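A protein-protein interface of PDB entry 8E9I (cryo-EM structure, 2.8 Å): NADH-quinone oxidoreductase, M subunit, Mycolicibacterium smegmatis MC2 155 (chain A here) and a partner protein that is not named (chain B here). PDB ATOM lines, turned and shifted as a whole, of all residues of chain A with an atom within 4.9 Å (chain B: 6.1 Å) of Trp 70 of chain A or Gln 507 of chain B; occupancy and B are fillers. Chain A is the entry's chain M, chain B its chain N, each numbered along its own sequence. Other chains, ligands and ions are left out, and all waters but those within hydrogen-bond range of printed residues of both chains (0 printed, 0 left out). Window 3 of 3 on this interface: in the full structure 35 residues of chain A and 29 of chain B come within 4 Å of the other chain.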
ATOM      1  N   HIS A  68      20.409 -31.097  32.576  1.00  0.00           N
ATOM      2  CA  HIS A  68      19.100 -30.701  33.072  1.00  0.00           C
ATOM      3  C   HIS A  68      18.032 -31.179  32.102  1.00  0.00           C
ATOM      4  O   HIS A  68      18.299 -31.394  30.919  1.00  0.00           O
ATOM      5  CB  HIS A  68      19.011 -29.185  33.259  1.00  0.00           C
ATOM      6  CG  HIS A  68      19.924 -28.653  34.317  1.00  0.00           C
ATOM      7  ND1 HIS A  68      19.524 -28.482  35.626  1.00  0.00           N
ATOM      8  CD2 HIS A  68      21.222 -28.272  34.267  1.00  0.00           C
ATOM      9  CE1 HIS A  68      20.533 -28.007  36.333  1.00  0.00           C
ATOM     10  NE2 HIS A  68      21.575 -27.872  35.534  1.00  0.00           N
ATOM     11  N   ARG A  69      16.818 -31.356  32.613  1.00  0.00           N
ATOM     12  CA  ARG A  69      15.704 -31.715  31.748  1.00  0.00           C
ATOM     13  C   ARG A  69      15.202 -30.478  31.021  1.00  0.00           C
ATOM     14  O   ARG A  69      14.978 -29.429  31.628  1.00  0.00           O
ATOM     15  CB  ARG A  69      14.577 -32.346  32.562  1.00  0.00           C
ATOM     16  N   TRP A  70      15.045 -30.598  29.704  1.00  0.00           N
ATOM     17  CA  TRP A  70      14.653 -29.457  28.888  1.00  0.00           C
ATOM     18  C   TRP A  70      13.336 -29.711  28.171  1.00  0.00           C
ATOM     19  O   TRP A  70      12.398 -28.919  28.289  1.00  0.00           O
ATOM     20  CB  TRP A  70      15.759 -29.142  27.888  1.00  0.00           C
ATOM     21  CG  TRP A  70      15.478 -27.985  27.014  1.00  0.00           C
ATOM     22  CD1 TRP A  70      14.886 -26.814  27.372  1.00  0.00           C
ATOM     23  CD2 TRP A  70      15.808 -27.865  25.629  1.00  0.00           C
ATOM     24  NE1 TRP A  70      14.813 -25.973  26.290  1.00  0.00           N
ATOM     25  CE2 TRP A  70      15.377 -26.595  25.207  1.00  0.00           C
ATOM     26  CE3 TRP A  70      16.424 -28.710  24.703  1.00  0.00           C
ATOM     27  CZ2 TRP A  70      15.540 -26.150  23.899  1.00  0.00           C
ATOM     28  CZ3 TRP A  70      16.585 -28.266  23.405  1.00  0.00           C
ATOM     29  CH2 TRP A  70      16.144 -26.997  23.015  1.00  0.00           C
ATOM     30  N   ILE A  71      13.253 -30.805  27.421  1.00  0.00           N
ATOM     31  CA  ILE A  71      12.018 -31.170  26.732  1.00  0.00           C
ATOM     32  C   ILE A  71      11.897 -32.690  26.758  1.00  0.00           C
ATOM     33  O   ILE A  71      12.159 -33.350  25.743  1.00  0.00           O
ATOM     34  CB  ILE A  71      11.992 -30.636  25.291  1.00  0.00           C
ATOM     35  CG1 ILE A  71      12.185 -29.120  25.261  1.00  0.00           C
ATOM     36  CG2 ILE A  71      10.669 -30.974  24.630  1.00  0.00           C
ATOM     37  CD1 ILE A  71      12.404 -28.564  23.869  1.00  0.00           C
ATOM     38  N   PRO A  72      11.514 -33.285  27.889  1.00  0.00           N
ATOM     39  CA  PRO A  72      11.395 -34.751  27.935  1.00  0.00           C
ATOM     40  C   PRO A  72      10.419 -35.311  26.919  1.00  0.00           C
ATOM     41  O   PRO A  72      10.572 -36.465  26.498  1.00  0.00           O
ATOM     42  CB  PRO A  72      10.924 -35.012  29.372  1.00  0.00           C
ATOM     43  CG  PRO A  72      11.418 -33.843  30.143  1.00  0.00           C
ATOM     44  CD  PRO A  72      11.319 -32.676  29.213  1.00  0.00           C
ATOM     45  N   SER A  73       9.413 -34.536  26.517  1.00  0.00           N
ATOM     46  CA  SER A  73       8.457 -35.030  25.533  1.00  0.00           C
ATOM     47  C   SER A  73       9.143 -35.399  24.228  1.00  0.00           C
ATOM     48  O   SER A  73       8.717 -36.338  23.547  1.00  0.00           O
ATOM     49  CB  SER A  73       7.372 -33.983  25.283  1.00  0.00           C
ATOM     50  OG  SER A  73       6.893 -33.447  26.505  1.00  0.00           O
ATOM     51  N   THR A  76      14.816 -34.946  24.592  1.00  0.00           N
ATOM     52  CA  THR A  76      16.011 -34.121  24.570  1.00  0.00           C
ATOM     53  C   THR A  76      16.140 -33.380  25.890  1.00  0.00           C
ATOM     54  O   THR A  76      15.145 -32.906  26.448  1.00  0.00           O
ATOM     55  CB  THR A  76      15.983 -33.112  23.424  1.00  0.00           C
ATOM     56  OG1 THR A  76      17.197 -32.352  23.432  1.00  0.00           O
ATOM     57  CG2 THR A  76      14.802 -32.164  23.566  1.00  0.00           C
ATOM     58  N   GLY A  77      17.369 -33.288  26.381  1.00  0.00           N
ATOM     59  CA  GLY A  77      17.647 -32.558  27.598  1.00  0.00           C
ATOM     60  C   GLY A  77      18.791 -31.586  27.418  1.00  0.00           C
ATOM     61  O   GLY A  77      19.654 -31.785  26.559  1.00  0.00           O
ATOM     62  N   TYR A  78      18.814 -30.533  28.230  1.00  0.00           N
ATOM     63  CA  TYR A  78      19.886 -29.545  28.180  1.00  0.00           C
ATOM     64  C   TYR A  78      21.127 -30.191  28.782  1.00  0.00           C
ATOM     65  O   TYR A  78      21.369 -30.150  29.991  1.00  0.00           O
ATOM     66  CB  TYR A  78      19.489 -28.280  28.926  1.00  0.00           C
ATOM     67  CG  TYR A  78      20.559 -27.223  28.952  1.00  0.00           C
ATOM     68  CD1 TYR A  78      20.675 -26.305  27.923  1.00  0.00           C
ATOM     69  CD2 TYR A  78      21.450 -27.137  30.007  1.00  0.00           C
ATOM     70  CE1 TYR A  78      21.649 -25.339  27.940  1.00  0.00           C
ATOM     71  CE2 TYR A  78      22.426 -26.174  30.035  1.00  0.00           C
ATOM     72  CZ  TYR A  78      22.521 -25.277  28.999  1.00  0.00           C
ATOM     73  OH  TYR A  78      23.496 -24.309  29.023  1.00  0.00           O
ATOM     74  N   LEU A 144      19.390 -30.557  20.868  1.00  0.00           N
ATOM     75  CA  LEU A 144      19.899 -29.246  21.259  1.00  0.00           C
ATOM     76  C   LEU A 144      20.933 -28.751  20.261  1.00  0.00           C
ATOM     77  O   LEU A 144      20.915 -27.584  19.837  1.00  0.00           O
ATOM     78  CB  LEU A 144      20.511 -29.322  22.656  1.00  0.00           C
ATOM     79  CG  LEU A 144      21.005 -27.993  23.226  1.00  0.00           C
ATOM     80  CD1 LEU A 144      19.834 -27.107  23.603  1.00  0.00           C
ATOM     81  CD2 LEU A 144      21.913 -28.234  24.415  1.00  0.00           C
ATOM     82  N   VAL A 147      19.211 -27.680  17.123  1.00  0.00           N
ATOM     83  CA  VAL A 147      18.586 -26.388  17.379  1.00  0.00           C
ATOM     84  C   VAL A 147      19.584 -25.269  17.136  1.00  0.00           C
ATOM     85  O   VAL A 147      19.368 -24.390  16.294  1.00  0.00           O
ATOM     86  CB  VAL A 147      18.031 -26.348  18.815  1.00  0.00           C
ATOM     87  CG1 VAL A 147      17.542 -24.961  19.189  1.00  0.00           C
ATOM     88  CG2 VAL A 147      16.893 -27.330  18.957  1.00  0.00           C
ATOM     89  N   LEU B 502       7.605 -19.693  23.976  1.00  0.00           N
ATOM     90  CA  LEU B 502       7.123 -21.022  23.647  1.00  0.00           C
ATOM     91  C   LEU B 502       8.004 -21.736  22.635  1.00  0.00           C
ATOM     92  O   LEU B 502       7.727 -22.893  22.311  1.00  0.00           O
ATOM     93  CB  LEU B 502       5.694 -20.913  23.115  1.00  0.00           C
ATOM     94  CG  LEU B 502       4.921 -22.205  22.875  1.00  0.00           C
ATOM     95  CD1 LEU B 502       4.932 -23.083  24.105  1.00  0.00           C
ATOM     96  CD2 LEU B 502       3.502 -21.872  22.475  1.00  0.00           C
ATOM     97  N   GLY B 503       9.039 -21.080  22.121  1.00  0.00           N
ATOM     98  CA  GLY B 503      10.003 -21.739  21.271  1.00  0.00           C
ATOM     99  C   GLY B 503      11.266 -22.061  22.034  1.00  0.00           C
ATOM    100  O   GLY B 503      11.890 -23.100  21.810  1.00  0.00           O
ATOM    101  N   ALA B 504      11.653 -21.170  22.946  1.00  0.00           N
ATOM    102  CA  ALA B 504      12.864 -21.407  23.723  1.00  0.00           C
ATOM    103  C   ALA B 504      12.630 -22.440  24.817  1.00  0.00           C
ATOM    104  O   ALA B 504      13.397 -23.401  24.944  1.00  0.00           O
ATOM    105  CB  ALA B 504      13.362 -20.097  24.329  1.00  0.00           C
ATOM    106  N   LEU B 505      11.570 -22.270  25.602  1.00  0.00           N
ATOM    107  CA  LEU B 505      11.260 -23.144  26.733  1.00  0.00           C
ATOM    108  C   LEU B 505       9.838 -23.652  26.563  1.00  0.00           C
ATOM    109  O   LEU B 505       8.917 -23.219  27.265  1.00  0.00           O
ATOM    110  CB  LEU B 505      11.428 -22.404  28.060  1.00  0.00           C
ATOM    111  N   PRO B 506       9.623 -24.578  25.627  1.00  0.00           N
ATOM    112  CA  PRO B 506       8.260 -25.017  25.315  1.00  0.00           C
ATOM    113  C   PRO B 506       7.694 -26.051  26.266  1.00  0.00           C
ATOM    114  O   PRO B 506       6.522 -26.415  26.113  1.00  0.00           O
ATOM    115  CB  PRO B 506       8.414 -25.617  23.918  1.00  0.00           C
ATOM    116  CG  PRO B 506       9.785 -26.175  23.934  1.00  0.00           C
ATOM    117  CD  PRO B 506      10.614 -25.210  24.743  1.00  0.00           C
ATOM    118  N   GLN B 507       8.470 -26.556  27.218  1.00  0.00           N
ATOM    119  CA  GLN B 507       7.972 -27.661  28.028  1.00  0.00           C
ATOM    120  C   GLN B 507       6.706 -27.241  28.763  1.00  0.00           C
ATOM    121  O   GLN B 507       5.766 -28.039  28.872  1.00  0.00           O
ATOM    122  CB  GLN B 507       9.030 -28.161  29.012  1.00  0.00           C
ATOM    123  CG  GLN B 507       8.564 -29.382  29.781  1.00  0.00           C
ATOM    124  CD  GLN B 507       8.146 -30.509  28.860  1.00  0.00           C
ATOM    125  OE1 GLN B 507       8.657 -30.636  27.749  1.00  0.00           O
ATOM    126  NE2 GLN B 507       7.191 -31.314  29.301  1.00  0.00           N
ATOM    127  N   PRO B 508       6.637 -26.029  29.304  1.00  0.00           N
ATOM    128  CA  PRO B 508       5.327 -25.489  29.666  1.00  0.00           C
ATOM    129  C   PRO B 508       4.438 -25.448  28.437  1.00  0.00           C
ATOM    130  O   PRO B 508       4.870 -25.075  27.347  1.00  0.00           O
ATOM    131  CB  PRO B 508       5.647 -24.088  30.192  1.00  0.00           C
ATOM    132  CG  PRO B 508       7.038 -24.195  30.690  1.00  0.00           C
ATOM    133  CD  PRO B 508       7.730 -25.156  29.763  1.00  0.00           C
ATOM    134  N   LEU B 509       3.189 -25.863  28.627  1.00  0.00           N
ATOM    135  CA  LEU B 509       2.192 -26.020  27.572  1.00  0.00           C
ATOM    136  C   LEU B 509       2.458 -27.247  26.713  1.00  0.00           C
ATOM    137  O   LEU B 509       1.523 -27.798  26.127  1.00  0.00           O
ATOM    138  CB  LEU B 509       2.144 -24.779  26.673  1.00  0.00           C
ATOM    139  CG  LEU B 509       1.209 -24.883  25.468  1.00  0.00           C
ATOM    140  CD1 LEU B 509      -0.227 -24.977  25.927  1.00  0.00           C
ATOM    141  CD2 LEU B 509       1.395 -23.702  24.548  1.00  0.00           C
ATOM    142  N   LEU B 510       3.671 -27.797  26.763  1.00  0.00           N
ATOM    143  CA  LEU B 510       3.900 -29.062  26.082  1.00  0.00           C
ATOM    144  C   LEU B 510       3.524 -30.215  26.991  1.00  0.00           C
ATOM    145  O   LEU B 510       2.994 -31.230  26.530  1.00  0.00           O
ATOM    146  CB  LEU B 510       5.353 -29.171  25.628  1.00  0.00           C
ATOM    147  CG  LEU B 510       5.674 -30.307  24.658  1.00  0.00           C
ATOM    148  CD1 LEU B 510       4.775 -30.254  23.440  1.00  0.00           C
ATOM    149  CD2 LEU B 510       7.125 -30.250  24.234  1.00  0.00           C
ATOM    150  N   ASP B 511       3.744 -30.052  28.293  1.00  0.00           N
ATOM    151  CA  ASP B 511       3.171 -30.986  29.250  1.00  0.00           C
ATOM    152  C   ASP B 511       1.651 -30.971  29.168  1.00  0.00           C
ATOM    153  O   ASP B 511       1.006 -32.023  29.251  1.00  0.00           O
ATOM    154  CB  ASP B 511       3.641 -30.640  30.661  1.00  0.00           C
ATOM    155  N   LEU B 512       1.057 -29.787  29.004  1.00  0.00           N
ATOM    156  CA  LEU B 512      -0.395 -29.699  28.883  1.00  0.00           C
ATOM    157  C   LEU B 512      -0.880 -30.331  27.585  1.00  0.00           C
ATOM    158  O   LEU B 512      -1.942 -30.961  27.552  1.00  0.00           O
ATOM    159  CB  LEU B 512      -0.843 -28.242  28.981  1.00  0.00           C
ATOM    160  CG  LEU B 512      -0.521 -27.542  30.304  1.00  0.00           C
ATOM    161  CD1 LEU B 512      -1.102 -26.137  30.327  1.00  0.00           C
ATOM    162  CD2 LEU B 512      -1.034 -28.345  31.489  1.00  0.00           C
ATOM    163  N   ASN B 514       0.620 -32.856  26.125  1.00  0.00           N
ATOM    164  CA  ASN B 514       0.721 -34.287  26.383  1.00  0.00           C
ATOM    165  C   ASN B 514      -0.457 -34.781  27.210  1.00  0.00           C
ATOM    166  O   ASN B 514      -1.073 -35.800  26.880  1.00  0.00           O
ATOM    167  CB  ASN B 514       2.034 -34.597  27.094  1.00  0.00           C
ATOM    168  CG  ASN B 514       3.237 -34.247  26.256  1.00  0.00           C
ATOM    169  OD1 ASN B 514       3.128 -34.054  25.045  1.00  0.00           O
ATOM    170  ND2 ASN B 514       4.397 -34.156  26.894  1.00  0.00           N
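The backbone carbonyl oxygen (O) of Leu 510 of chain B lies close to the side-chain amide oxygen (OD1) of Asn 514 of chain B.
The backbone NH (N) of Ile 71 of chain A sits at hydrogen-bond distance from the backbone carbonyl oxygen (O) of Thr 76 of chain A, 3.0 Å away.
Among the printed residues, merely in contact across the chains: Trp 70 of chain A with Gln 507 of chain B (3.5 Å), Ile 71 of chain A with Pro 506 of chain B (3.5 Å), Ile 71 of chain A with Gln 507 of chain B (3.6 Å), Ile 71 of chain A with Leu 510 of chain B (3.6 Å), Pro 72 of chain A with Gln 507 of chain B (3.7 Å), Ser 73 of chain A with Gln 507 of chain B (3.5 Å) and Ser 73 of chain A with Leu 510 of chain B (3.8 Å).
Of the printed residues of chain B, Trp 70 of chain A touches Ala 504 and Gln 507.
Gln 507 of chain B touches just these residues of chain A: Trp 70 (3.5 Å), Ile 71 (3.6 Å), Pro 72 (3.7 Å) and Ser 73 (3.5 Å).
Of the printed residues of chain B, Pro 72 of chain A touches Gln 507.
Printed residues of chain B within 4 Å of Ser 73 of chain A: Gln 507, Leu 510 and Asn 514.
Of the printed residues of chain A, Leu 510 of chain B touches Ile 71 and Ser 73.
Leu 505 of chain B touches none of the printed residues of chain A.
The nearest printed residue of chain B that does not touch Trp 70 of chain A is Pro 506 of chain B (4.5 Å).
The nearest printed residue of chain A that does not touch Asn 514 of chain B is Pro 72 of chain A (6.1 Å).
The backbone carbonyl oxygen (O) of Ala 504 of chain B sits at hydrogen-bond distance from the indole nitrogen (NE1) of Trp 70 of chain A, 3.2 Å away.
The side-chain amide nitrogen (ND2) of Asn 514 of chain B sits at hydrogen-bond distance from the side-chain hydroxyl (OG) of Ser 73 of chain A (2.6 Å).
Hydrophobic or aromatic side chains of chain B within 4 Å of the printed part of chain A: Pro 506 and Leu 510.
Printed residues of chain A that touch a printed residue of chain B: Trp 70, Ile 71, Pro 72 and Ser 73.
Hydrophobic or aromatic side chains of chain A within 4 Å of the printed part of chain B: Trp 70, Ile 71 and Pro 72.
Among the printed residues, 9 pairs touch across the chains.
Among the printed residues, no Asp or Glu carboxylate lies within 4 Å of a Lys or Arg side-chain nitrogen of the other chain.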
